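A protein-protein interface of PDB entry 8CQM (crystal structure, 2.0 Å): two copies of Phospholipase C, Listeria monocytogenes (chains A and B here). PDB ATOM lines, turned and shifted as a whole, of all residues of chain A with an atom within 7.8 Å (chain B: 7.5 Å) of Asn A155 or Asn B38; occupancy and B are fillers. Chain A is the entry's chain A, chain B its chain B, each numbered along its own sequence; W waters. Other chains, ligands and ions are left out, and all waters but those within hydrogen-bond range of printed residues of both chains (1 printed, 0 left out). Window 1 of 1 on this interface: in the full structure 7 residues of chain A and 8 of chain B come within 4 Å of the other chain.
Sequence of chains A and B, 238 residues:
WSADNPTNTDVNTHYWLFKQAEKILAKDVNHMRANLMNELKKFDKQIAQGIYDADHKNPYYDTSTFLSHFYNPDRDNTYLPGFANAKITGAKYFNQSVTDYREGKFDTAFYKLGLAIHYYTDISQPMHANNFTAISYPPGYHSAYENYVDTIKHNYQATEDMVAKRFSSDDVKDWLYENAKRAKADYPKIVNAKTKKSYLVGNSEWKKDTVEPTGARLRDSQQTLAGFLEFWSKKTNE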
ATOM      1  N   TRP A  16      28.846  -6.688  -8.716  1.00  0.00           N
ATOM      2  CA  TRP A  16      28.340  -6.527  -7.358  1.00  0.00           C
ATOM      3  C   TRP A  16      26.860  -6.889  -7.288  1.00  0.00           C
ATOM      4  O   TRP A  16      26.429  -7.569  -6.351  1.00  0.00           O
ATOM      5  CB  TRP A  16      28.584  -5.090  -6.893  1.00  0.00           C
ATOM      6  CG  TRP A  16      28.044  -4.744  -5.544  1.00  0.00           C
ATOM      7  CD1 TRP A  16      28.691  -4.870  -4.325  1.00  0.00           C
ATOM      8  CD2 TRP A  16      26.763  -4.177  -5.255  1.00  0.00           C
ATOM      9  NE1 TRP A  16      27.886  -4.417  -3.316  1.00  0.00           N
ATOM     10  CE2 TRP A  16      26.695  -3.988  -3.856  1.00  0.00           C
ATOM     11  CE3 TRP A  16      25.665  -3.803  -6.047  1.00  0.00           C
ATOM     12  CZ2 TRP A  16      25.565  -3.463  -3.227  1.00  0.00           C
ATOM     13  CZ3 TRP A  16      24.552  -3.266  -5.417  1.00  0.00           C
ATOM     14  CH2 TRP A  16      24.518  -3.091  -4.018  1.00  0.00           C
ATOM     15  N   VAL A 149      27.725   6.000  -8.128  1.00  0.00           N
ATOM     16  CA  VAL A 149      27.019   4.813  -7.659  1.00  0.00           C
ATOM     17  C   VAL A 149      28.009   3.746  -7.219  1.00  0.00           C
ATOM     18  O   VAL A 149      27.814   3.076  -6.200  1.00  0.00           O
ATOM     19  CB  VAL A 149      26.096   4.269  -8.762  1.00  0.00           C
ATOM     20  CG1 VAL A 149      25.571   2.894  -8.369  1.00  0.00           C
ATOM     21  CG2 VAL A 149      24.970   5.233  -9.049  1.00  0.00           C
ATOM     22  N   ASP A 150      29.057   3.543  -8.013  1.00  0.00           N
ATOM     23  CA  ASP A 150      30.101   2.589  -7.658  1.00  0.00           C
ATOM     24  C   ASP A 150      30.664   2.861  -6.269  1.00  0.00           C
ATOM     25  O   ASP A 150      30.950   1.922  -5.519  1.00  0.00           O
ATOM     26  CB  ASP A 150      31.225   2.628  -8.692  1.00  0.00           C
ATOM     27  CG  ASP A 150      32.328   1.608  -8.403  1.00  0.00           C
ATOM     28  OD1 ASP A 150      32.080   0.392  -8.525  1.00  0.00           O
ATOM     29  OD2 ASP A 150      33.435   2.036  -8.023  1.00  0.00           O
ATOM     30  N   THR A 151      30.855   4.132  -5.914  1.00  0.00           N
ATOM     31  CA  THR A 151      31.493   4.405  -4.635  1.00  0.00           C
ATOM     32  C   THR A 151      30.550   4.181  -3.463  1.00  0.00           C
ATOM     33  O   THR A 151      31.031   3.969  -2.352  1.00  0.00           O
ATOM     34  CB  THR A 151      32.047   5.843  -4.535  1.00  0.00           C
ATOM     35  OG1 THR A 151      30.980   6.759  -4.292  1.00  0.00           O
ATOM     36  CG2 THR A 151      32.812   6.269  -5.775  1.00  0.00           C
ATOM     37  N   ILE A 152      29.226   4.217  -3.667  1.00  0.00           N
ATOM     38  CA  ILE A 152      28.299   4.145  -2.543  1.00  0.00           C
ATOM     39  C   ILE A 152      27.447   2.881  -2.542  1.00  0.00           C
ATOM     40  O   ILE A 152      26.669   2.685  -1.597  1.00  0.00           O
ATOM     41  CB  ILE A 152      27.409   5.404  -2.467  1.00  0.00           C
ATOM     42  CG1 ILE A 152      26.680   5.670  -3.789  1.00  0.00           C
ATOM     43  CG2 ILE A 152      28.248   6.627  -2.143  1.00  0.00           C
ATOM     44  CD1 ILE A 152      25.389   4.977  -3.933  1.00  0.00           C
ATOM     45  N   LYS A 153      27.575   2.007  -3.550  1.00  0.00           N
ATOM     46  CA  LYS A 153      26.726   0.820  -3.592  1.00  0.00           C
ATOM     47  C   LYS A 153      26.886  -0.045  -2.346  1.00  0.00           C
ATOM     48  O   LYS A 153      25.919  -0.702  -1.926  1.00  0.00           O
ATOM     49  CB  LYS A 153      27.002  -0.006  -4.855  1.00  0.00           C
ATOM     50  CG  LYS A 153      28.403  -0.630  -4.941  1.00  0.00           C
ATOM     51  CD  LYS A 153      28.682  -1.163  -6.337  1.00  0.00           C
ATOM     52  CE  LYS A 153      30.057  -1.855  -6.407  1.00  0.00           C
ATOM     53  NZ  LYS A 153      31.209  -0.987  -5.918  1.00  0.00           N
ATOM     54  N   HIS A 154      28.068  -0.032  -1.715  1.00  0.00           N
ATOM     55  CA  HIS A 154      28.306  -0.907  -0.571  1.00  0.00           C
ATOM     56  C   HIS A 154      27.394  -0.580   0.604  1.00  0.00           C
ATOM     57  O   HIS A 154      27.263  -1.402   1.519  1.00  0.00           O
ATOM     58  CB  HIS A 154      29.776  -0.841  -0.126  1.00  0.00           C
ATOM     59  CG  HIS A 154      30.190   0.480   0.451  1.00  0.00           C
ATOM     60  ND1 HIS A 154      30.511   1.572  -0.329  1.00  0.00           N
ATOM     61  CD2 HIS A 154      30.400   0.864   1.734  1.00  0.00           C
ATOM     62  CE1 HIS A 154      30.871   2.579   0.449  1.00  0.00           C
ATOM     63  NE2 HIS A 154      30.803   2.180   1.707  1.00  0.00           N
ATOM     64  N   ASN A 155      26.757   0.582   0.596  1.00  0.00           N
ATOM     65  CA  ASN A 155      25.752   0.916   1.599  1.00  0.00           C
ATOM     66  C   ASN A 155      24.373   0.337   1.310  1.00  0.00           C
ATOM     67  O   ASN A 155      23.455   0.568   2.113  1.00  0.00           O
ATOM     68  CB  ASN A 155      25.650   2.434   1.757  1.00  0.00           C
ATOM     69  CG  ASN A 155      26.881   3.010   2.406  1.00  0.00           C
ATOM     70  OD1 ASN A 155      27.418   2.425   3.347  1.00  0.00           O
ATOM     71  ND2 ASN A 155      27.341   4.143   1.906  1.00  0.00           N
ATOM     72  N   TYR A 156      24.195  -0.385   0.197  1.00  0.00           N
ATOM     73  CA  TYR A 156      22.903  -0.956  -0.185  1.00  0.00           C
ATOM     74  C   TYR A 156      23.048  -2.417  -0.550  1.00  0.00           C
ATOM     75  O   TYR A 156      22.467  -2.896  -1.528  1.00  0.00           O
ATOM     76  CB  TYR A 156      22.268  -0.167  -1.331  1.00  0.00           C
ATOM     77  CG  TYR A 156      22.146   1.283  -0.955  1.00  0.00           C
ATOM     78  CD1 TYR A 156      21.118   1.718  -0.151  1.00  0.00           C
ATOM     79  CD2 TYR A 156      23.102   2.196  -1.343  1.00  0.00           C
ATOM     80  CE1 TYR A 156      21.023   3.030   0.218  1.00  0.00           C
ATOM     81  CE2 TYR A 156      23.013   3.506  -0.996  1.00  0.00           C
ATOM     82  CZ  TYR A 156      21.973   3.920  -0.205  1.00  0.00           C
ATOM     83  OH  TYR A 156      21.890   5.239   0.161  1.00  0.00           O
ATOM     84  N   GLN A 157      23.792  -3.159   0.266  1.00  0.00           N
ATOM     85  CA  GLN A 157      23.971  -4.594   0.089  1.00  0.00           C
ATOM     86  C   GLN A 157      22.667  -5.347   0.408  1.00  0.00           C
ATOM     87  O   GLN A 157      21.703  -4.791   0.941  1.00  0.00           O
ATOM     88  CB  GLN A 157      25.116  -5.094   0.973  1.00  0.00           C
ATOM     89  CG  GLN A 157      26.479  -4.584   0.511  1.00  0.00           C
ATOM     90  CD  GLN A 157      27.623  -4.991   1.431  1.00  0.00           C
ATOM     91  OE1 GLN A 157      27.936  -6.178   1.543  1.00  0.00           O
ATOM     92  NE2 GLN A 157      28.270  -4.001   2.075  1.00  0.00           N
ATOM     93  N   ALA A 158      22.656  -6.627   0.054  1.00  0.00           N
ATOM     94  CA  ALA A 158      21.474  -7.459   0.245  1.00  0.00           C
ATOM     95  C   ALA A 158      21.154  -7.600   1.726  1.00  0.00           C
ATOM     96  O   ALA A 158      22.058  -7.668   2.560  1.00  0.00           O
ATOM     97  CB  ALA A 158      21.706  -8.833  -0.376  1.00  0.00           C
ATOM     98  N   THR A 159      19.862  -7.592   2.061  1.00  0.00           N
ATOM     99  CA  THR A 159      19.436  -7.754   3.446  1.00  0.00           C
ATOM    100  C   THR A 159      18.440  -8.906   3.544  1.00  0.00           C
ATOM    101  O   THR A 159      17.830  -9.314   2.552  1.00  0.00           O
ATOM    102  CB  THR A 159      18.831  -6.458   3.992  1.00  0.00           C
ATOM    103  OG1 THR A 159      17.710  -6.075   3.186  1.00  0.00           O
ATOM    104  CG2 THR A 159      19.850  -5.342   3.941  1.00  0.00           C
ATOM    105  N   VAL A 211      21.173   9.893  -3.910  1.00  0.00           N
ATOM    106  CA  VAL A 211      21.653   8.749  -3.132  1.00  0.00           C
ATOM    107  C   VAL A 211      20.490   7.835  -2.722  1.00  0.00           C
ATOM    108  O   VAL A 211      20.548   6.616  -2.919  1.00  0.00           O
ATOM    109  CB  VAL A 211      22.485   9.227  -1.923  1.00  0.00           C
ATOM    110  CG1 VAL A 211      21.679  10.098  -1.029  1.00  0.00           C
ATOM    111  CG2 VAL A 211      23.035   8.026  -1.145  1.00  0.00           C
ATOM    112  N   GLU A 212      19.398   8.399  -2.193  1.00  0.00           N
ATOM    113  CA  GLU A 212      18.304   7.523  -1.766  1.00  0.00           C
ATOM    114  C   GLU A 212      17.575   6.869  -2.937  1.00  0.00           C
ATOM    115  O   GLU A 212      17.387   5.641  -2.901  1.00  0.00           O
ATOM    116  CB  GLU A 212      17.339   8.275  -0.843  1.00  0.00           C
ATOM    117  CG  GLU A 212      17.845   8.355   0.615  1.00  0.00           C
ATOM    118  CD  GLU A 212      18.246   6.984   1.180  1.00  0.00           C
ATOM    119  OE1 GLU A 212      17.351   6.123   1.365  1.00  0.00           O
ATOM    120  OE2 GLU A 212      19.453   6.756   1.430  1.00  0.00           O
ATOM    121  N   GLY A 215      19.751   4.076  -3.986  1.00  0.00           N
ATOM    122  CA  GLY A 215      19.727   2.925  -3.107  1.00  0.00           C
ATOM    123  C   GLY A 215      18.512   2.059  -3.353  1.00  0.00           C
ATOM    124  O   GLY A 215      18.606   0.827  -3.373  1.00  0.00           O
ATOM    125  N   LEU A 218      19.083   0.147  -6.696  1.00  0.00           N
ATOM    126  CA  LEU A 218      19.998  -0.982  -6.499  1.00  0.00           C
ATOM    127  C   LEU A 218      19.334  -2.123  -5.740  1.00  0.00           C
ATOM    128  O   LEU A 218      19.551  -3.297  -6.057  1.00  0.00           O
ATOM    129  CB  LEU A 218      21.255  -0.531  -5.762  1.00  0.00           C
ATOM    130  CG  LEU A 218      22.178   0.405  -6.527  1.00  0.00           C
ATOM    131  CD1 LEU A 218      23.259   0.900  -5.598  1.00  0.00           C
ATOM    132  CD2 LEU A 218      22.768  -0.323  -7.710  1.00  0.00           C
ATOM    133  N   ARG A 219      18.539  -1.802  -4.725  1.00  0.00           N
ATOM    134  CA  ARG A 219      17.849  -2.854  -3.985  1.00  0.00           C
ATOM    135  C   ARG A 219      16.799  -3.550  -4.850  1.00  0.00           C
ATOM    136  O   ARG A 219      16.646  -4.777  -4.794  1.00  0.00           O
ATOM    137  CB  ARG A 219      17.201  -2.254  -2.725  1.00  0.00           C
ATOM    138  CG  ARG A 219      18.224  -1.856  -1.619  1.00  0.00           C
ATOM    139  CD  ARG A 219      17.560  -1.303  -0.329  1.00  0.00           C
ATOM    140  NE  ARG A 219      16.397  -2.095   0.064  1.00  0.00           N
ATOM    141  CZ  ARG A 219      16.377  -3.014   1.028  1.00  0.00           C
ATOM    142  NH1 ARG A 219      17.448  -3.275   1.768  1.00  0.00           N
ATOM    143  NH2 ARG A 219      15.258  -3.706   1.238  1.00  0.00           N
ATOM    144  N   GLN A 222      18.850  -5.831  -7.457  1.00  0.00           N
ATOM    145  CA  GLN A 222      19.354  -7.078  -6.865  1.00  0.00           C
ATOM    146  C   GLN A 222      18.278  -8.137  -6.841  1.00  0.00           C
ATOM    147  O   GLN A 222      18.532  -9.315  -7.122  1.00  0.00           O
ATOM    148  CB  GLN A 222      19.791  -6.881  -5.408  1.00  0.00           C
ATOM    149  CG  GLN A 222      20.905  -6.018  -5.185  1.00  0.00           C
ATOM    150  CD  GLN A 222      20.971  -5.621  -3.732  1.00  0.00           C
ATOM    151  OE1 GLN A 222      20.871  -6.460  -2.810  1.00  0.00           O
ATOM    152  NE2 GLN A 222      21.052  -4.341  -3.517  1.00  0.00           N
ATOM    153  N   VAL B  29      21.279  12.723   4.069  1.00  0.00           N
ATOM    154  CA  VAL B  29      22.391  11.796   4.235  1.00  0.00           C
ATOM    155  C   VAL B  29      23.715  12.551   4.301  1.00  0.00           C
ATOM    156  O   VAL B  29      23.899  13.602   3.669  1.00  0.00           O
ATOM    157  CB  VAL B  29      22.408  10.776   3.084  1.00  0.00           C
ATOM    158  CG1 VAL B  29      23.637   9.905   3.208  1.00  0.00           C
ATOM    159  CG2 VAL B  29      21.145   9.925   3.103  1.00  0.00           C
ATOM    160  N   ASN B  30      24.643  11.953   5.059  1.00  0.00           N
ATOM    161  CA  ASN B  30      26.042  12.421   5.194  1.00  0.00           C
ATOM    162  C   ASN B  30      26.875  11.135   5.331  1.00  0.00           C
ATOM    163  O   ASN B  30      26.271  10.054   5.404  1.00  0.00           O
ATOM    164  CB  ASN B  30      26.230  13.363   6.377  1.00  0.00           C
ATOM    165  CG  ASN B  30      26.138  12.721   7.742  1.00  0.00           C
ATOM    166  OD1 ASN B  30      26.704  11.662   7.991  1.00  0.00           O
ATOM    167  ND2 ASN B  30      25.456  13.394   8.652  1.00  0.00           N
ATOM    168  N   HIS B  31      28.197  11.228   5.435  1.00  0.00           N
ATOM    169  CA  HIS B  31      29.054  10.008   5.457  1.00  0.00           C
ATOM    170  C   HIS B  31      28.724   9.033   6.597  1.00  0.00           C
ATOM    171  O   HIS B  31      28.540   7.852   6.321  1.00  0.00           O
ATOM    172  CB  HIS B  31      30.540  10.397   5.520  1.00  0.00           C
ATOM    173  CG  HIS B  31      31.445   9.245   5.764  1.00  0.00           C
ATOM    174  ND1 HIS B  31      32.305   9.205   6.836  1.00  0.00           N
ATOM    175  CD2 HIS B  31      31.614   8.091   5.089  1.00  0.00           C
ATOM    176  CE1 HIS B  31      32.971   8.074   6.812  1.00  0.00           C
ATOM    177  NE2 HIS B  31      32.568   7.376   5.751  1.00  0.00           N
ATOM    178  N   MET B  32      28.718   9.516   7.839  1.00  0.00           N
ATOM    179  CA  MET B  32      28.524   8.587   8.976  1.00  0.00           C
ATOM    180  C   MET B  32      27.077   8.092   8.955  1.00  0.00           C
ATOM    181  O   MET B  32      26.864   6.913   9.273  1.00  0.00           O
ATOM    182  CB  MET B  32      28.841   9.252  10.317  1.00  0.00           C
ATOM    183  CG  MET B  32      30.318   9.249  10.696  1.00  0.00           C
ATOM    184  SD  MET B  32      31.342   7.932   9.972  1.00  0.00           S
ATOM    185  CE  MET B  32      30.941   6.554  11.044  1.00  0.00           C
ATOM    186  N   ARG B  33      26.131   8.931   8.529  1.00  0.00           N
ATOM    187  CA  ARG B  33      24.783   8.397   8.572  1.00  0.00           C
ATOM    188  C   ARG B  33      24.590   7.306   7.534  1.00  0.00           C
ATOM    189  O   ARG B  33      23.788   6.394   7.750  1.00  0.00           O
ATOM    190  CB  ARG B  33      23.781   9.520   8.332  1.00  0.00           C
ATOM    191  CG  ARG B  33      23.694  10.548   9.449  1.00  0.00           C
ATOM    192  CD  ARG B  33      22.639  11.569   9.059  1.00  0.00           C
ATOM    193  NE  ARG B  33      22.306  12.501  10.128  1.00  0.00           N
ATOM    194  CZ  ARG B  33      21.378  13.443  10.021  1.00  0.00           C
ATOM    195  NH1 ARG B  33      20.698  13.617   8.898  1.00  0.00           N
ATOM    196  NH2 ARG B  33      21.113  14.216  11.072  1.00  0.00           N
ATOM    197  N   ALA B  34      25.340   7.354   6.429  1.00  0.00           N
ATOM    198  CA  ALA B  34      25.174   6.339   5.397  1.00  0.00           C
ATOM    199  C   ALA B  34      25.594   4.973   5.935  1.00  0.00           C
ATOM    200  O   ALA B  34      24.909   3.968   5.713  1.00  0.00           O
ATOM    201  CB  ALA B  34      25.975   6.713   4.152  1.00  0.00           C
ATOM    202  N   ASN B  35      26.696   4.934   6.692  1.00  0.00           N
ATOM    203  CA  ASN B  35      27.153   3.681   7.286  1.00  0.00           C
ATOM    204  C   ASN B  35      26.166   3.166   8.322  1.00  0.00           C
ATOM    205  O   ASN B  35      25.878   1.967   8.365  1.00  0.00           O
ATOM    206  CB  ASN B  35      28.523   3.880   7.939  1.00  0.00           C
ATOM    207  CG  ASN B  35      29.608   4.089   6.917  1.00  0.00           C
ATOM    208  OD1 ASN B  35      30.377   5.056   6.998  1.00  0.00           O
ATOM    209  ND2 ASN B  35      29.662   3.192   5.916  1.00  0.00           N
ATOM    210  N   LEU B  36      25.646   4.065   9.167  1.00  0.00           N
ATOM    211  CA  LEU B  36      24.666   3.671  10.173  1.00  0.00           C
ATOM    212  C   LEU B  36      23.403   3.121   9.521  1.00  0.00           C
ATOM    213  O   LEU B  36      22.890   2.079   9.933  1.00  0.00           O
ATOM    214  CB  LEU B  36      24.331   4.862  11.069  1.00  0.00           C
ATOM    215  CG  LEU B  36      23.159   4.643  12.033  1.00  0.00           C
ATOM    216  CD1 LEU B  36      23.538   3.565  13.048  1.00  0.00           C
ATOM    217  CD2 LEU B  36      22.772   5.943  12.728  1.00  0.00           C
ATOM    218  N   MET B  37      22.898   3.815   8.490  1.00  0.00           N
ATOM    219  CA  MET B  37      21.679   3.387   7.804  1.00  0.00           C
ATOM    220  C   MET B  37      21.822   2.006   7.185  1.00  0.00           C
ATOM    221  O   MET B  37      20.876   1.207   7.219  1.00  0.00           O
ATOM    222  CB  MET B  37      21.276   4.402   6.732  1.00  0.00           C
ATOM    223  CG  MET B  37      20.632   5.684   7.255  1.00  0.00           C
ATOM    224  SD  MET B  37      19.323   5.287   8.461  1.00  0.00           S
ATOM    225  CE  MET B  37      18.233   4.199   7.535  1.00  0.00           C
ATOM    226  N   ASN B  38      22.986   1.702   6.613  1.00  0.00           N
ATOM    227  CA  ASN B  38      23.170   0.366   6.050  1.00  0.00           C
ATOM    228  C   ASN B  38      23.079  -0.706   7.138  1.00  0.00           C
ATOM    229  O   ASN B  38      22.452  -1.752   6.933  1.00  0.00           O
ATOM    230  CB  ASN B  38      24.515   0.296   5.314  1.00  0.00           C
ATOM    231  CG  ASN B  38      24.917  -1.135   4.924  1.00  0.00           C
ATOM    232  OD1 ASN B  38      24.273  -1.795   4.084  1.00  0.00           O
ATOM    233  ND2 ASN B  38      25.996  -1.607   5.515  1.00  0.00           N
ATOM    234  N   GLU B  39      23.658  -0.442   8.316  1.00  0.00           N
ATOM    235  CA  GLU B  39      23.574  -1.369   9.450  1.00  0.00           C
ATOM    236  C   GLU B  39      22.142  -1.537   9.955  1.00  0.00           C
ATOM    237  O   GLU B  39      21.691  -2.659  10.230  1.00  0.00           O
ATOM    238  CB  GLU B  39      24.458  -0.871  10.590  1.00  0.00           C
ATOM    239  CG  GLU B  39      25.922  -0.902  10.281  1.00  0.00           C
ATOM    240  CD  GLU B  39      26.759  -0.388  11.434  1.00  0.00           C
ATOM    241  OE1 GLU B  39      26.242   0.417  12.253  1.00  0.00           O
ATOM    242  OE2 GLU B  39      27.941  -0.765  11.508  1.00  0.00           O
ATOM    243  N   LEU B  40      21.437  -0.423  10.157  1.00  0.00           N
ATOM    244  CA  LEU B  40      20.070  -0.497  10.656  1.00  0.00           C
ATOM    245  C   LEU B  40      19.184  -1.293   9.710  1.00  0.00           C
ATOM    246  O   LEU B  40      18.300  -2.035  10.150  1.00  0.00           O
ATOM    247  CB  LEU B  40      19.510   0.906  10.851  1.00  0.00           C
ATOM    248  CG  LEU B  40      20.251   1.846  11.807  1.00  0.00           C
ATOM    249  CD1 LEU B  40      19.549   3.206  11.741  1.00  0.00           C
ATOM    250  CD2 LEU B  40      20.289   1.298  13.230  1.00  0.00           C
ATOM    251  N   LYS B  41      19.414  -1.160   8.403  1.00  0.00           N
ATOM    252  CA  LYS B  41      18.639  -1.925   7.436  1.00  0.00           C
ATOM    253  C   LYS B  41      19.001  -3.406   7.519  1.00  0.00           C
ATOM    254  O   LYS B  41      18.118  -4.271   7.578  1.00  0.00           O
ATOM    255  CB  LYS B  41      18.893  -1.375   6.028  1.00  0.00           C
ATOM    256  CG  LYS B  41      18.007  -1.940   4.957  1.00  0.00           C
ATOM    257  CD  LYS B  41      16.609  -1.330   5.098  1.00  0.00           C
ATOM    258  CE  LYS B  41      15.641  -1.848   4.056  1.00  0.00           C
ATOM    259  NZ  LYS B  41      15.346  -3.290   4.260  1.00  0.00           N
ATOM    260  N   LYS B  42      20.299  -3.711   7.579  1.00  0.00           N
ATOM    261  CA  LYS B  42      20.733  -5.107   7.583  1.00  0.00           C
ATOM    262  C   LYS B  42      20.281  -5.832   8.852  1.00  0.00           C
ATOM    263  O   LYS B  42      19.915  -7.015   8.805  1.00  0.00           O
ATOM    264  CB  LYS B  42      22.253  -5.165   7.411  1.00  0.00           C
ATOM    265  CG  LYS B  42      22.865  -6.544   7.587  1.00  0.00           C
ATOM    266  CD  LYS B  42      24.328  -6.591   7.102  1.00  0.00           C
ATOM    267  CE  LYS B  42      25.030  -5.250   7.309  1.00  0.00           C
ATOM    268  NZ  LYS B  42      26.504  -5.348   7.160  1.00  0.00           N
ATOM    269  N   PHE B  43      20.280  -5.136   9.991  1.00  0.00           N
ATOM    270  CA  PHE B  43      19.915  -5.720  11.276  1.00  0.00           C
ATOM    271  C   PHE B  43      18.502  -5.331  11.721  1.00  0.00           C
ATOM    272  O   PHE B  43      18.202  -5.319  12.924  1.00  0.00           O
ATOM    273  CB  PHE B  43      20.950  -5.320  12.327  1.00  0.00           C
ATOM    274  CG  PHE B  43      22.286  -5.986  12.128  1.00  0.00           C
ATOM    275  CD1 PHE B  43      22.521  -7.266  12.618  1.00  0.00           C
ATOM    276  CD2 PHE B  43      23.294  -5.352  11.408  1.00  0.00           C
ATOM    277  CE1 PHE B  43      23.752  -7.872  12.427  1.00  0.00           C
ATOM    278  CE2 PHE B  43      24.514  -5.963  11.220  1.00  0.00           C
ATOM    279  CZ  PHE B  43      24.742  -7.218  11.723  1.00  0.00           C
ATOM    280  N   ASP B  44      17.620  -5.015  10.773  1.00  0.00           N
ATOM    281  CA  ASP B  44      16.268  -4.607  11.143  1.00  0.00           C
ATOM    282  C   ASP B  44      15.563  -5.662  11.991  1.00  0.00           C
ATOM    283  O   ASP B  44      14.869  -5.329  12.959  1.00  0.00           O
ATOM    284  CB  ASP B  44      15.440  -4.303   9.902  1.00  0.00           C
ATOM    285  CG  ASP B  44      14.077  -3.764  10.257  1.00  0.00           C
ATOM    286  OD1 ASP B  44      14.002  -2.583  10.610  1.00  0.00           O
ATOM    287  OD2 ASP B  44      13.095  -4.529  10.234  1.00  0.00           O
ATOM    288  N   PHE B 110      22.784  -5.420  18.055  1.00  0.00           N
ATOM    289  CA  PHE B 110      21.625  -4.758  17.474  1.00  0.00           C
ATOM    290  C   PHE B 110      20.324  -5.150  18.160  1.00  0.00           C
ATOM    291  O   PHE B 110      19.394  -4.333  18.220  1.00  0.00           O
ATOM    292  CB  PHE B 110      21.572  -5.003  15.961  1.00  0.00           C
ATOM    293  CG  PHE B 110      22.547  -4.137  15.207  1.00  0.00           C
ATOM    294  CD1 PHE B 110      22.251  -2.812  14.957  1.00  0.00           C
ATOM    295  CD2 PHE B 110      23.772  -4.630  14.799  1.00  0.00           C
ATOM    296  CE1 PHE B 110      23.146  -1.989  14.290  1.00  0.00           C
ATOM    297  CE2 PHE B 110      24.676  -3.812  14.144  1.00  0.00           C
ATOM    298  CZ  PHE B 110      24.363  -2.497  13.883  1.00  0.00           C
HETATM  299  O   HOH W   1      22.703   3.138   3.562  1.00  0.00           O
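Among the printed residues, merely in contact across the chains: His A154 with Asn B38 (3.96 Å), Asn A155 with Ala B34 (3.7 Å), Thr A159 with Lys B41 (3.8 Å), Thr A159 with Lys B42 (3.8 Å) and Glu A212 with Val B29 (3.96 Å).
OD1 of Asn A155 is in hydrogen-bond range of ND2 of Asn B35, at 3.5 Å.
O of Asn A155 lies close to OD1 of Asn B38.
The side-chain amino group (NZ) of Lys B41 sits close to the guanidinium group (NH2) of Arg A219 (3.1 Å).
No position is printed for both chains.
Of the 8 pairs that touch across the chains among the printed residues, none has its exchanged pair printed and touching as well.
O of Thr A151 lies close to ND1 of His A154 (3.2 Å).
The backbone carbonyl oxygen of His A154 is in hydrogen-bond range of the side-chain amide nitrogen of Gln A157 (2.8 Å).
The side-chain carboxylate of Glu A212 lies within hydrogen-bond range of the side-chain hydroxyl of Tyr A156 (3.1 Å).
The guanidinium group (NH1) of Arg A219 sits at hydrogen-bond distance from the side-chain hydroxyl (OG1) of Thr A159, at 3.1 Å.
The side-chain amide oxygen (OD1) of Asn B35 sits close to the backbone carbonyl oxygen (O) of His B31 (3.4 Å).
Printed residues of chain B that touch a printed residue of chain A: Val B29, Ala B34, Asn B35, Asn B38, Lys B41 and Lys B42.
Hydrophobic or aromatic side chains of chain B that line the printed part of chain A: Val B29 and Ala B34.
Of the printed residues of chain B, His A154 touches Asn B38.
Asn A155 touches just these residues of chain B: Ala B34 (3.7 Å), Asn B35 (3.5 Å) and Asn B38 (3.2 Å).
Of the printed residues of chain B, Thr A159 touches Lys B41 (3.8 Å) and Lys B42 (3.8 Å).
Of the printed residues of chain A, Asn B35 touches Asn A155 (3.5 Å).
Asn B38 touches just these residues of chain A: His A154 and Asn A155.
Of the printed residues of chain A, Lys B41 touches Thr A159 and Arg A219.
Of the printed residues of chain A, Lys B42 touches Thr A159 (3.8 Å).
The nearest residue of chain B that does not touch Asn A155 is Met B37 (5.5 Å).
The nearest residue of chain A that does not touch Asn B38 is Gln A157 (4.1 Å).
The nearest printed residue of chain B that does not touch Thr A159 is Asn B38 (5.3 Å).
Water W1 lies within hydrogen-bond range of O of Asn A155 (3.0 Å), O of Ala B34 (3.2 Å) and N of Asn B38 (3.4 Å).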
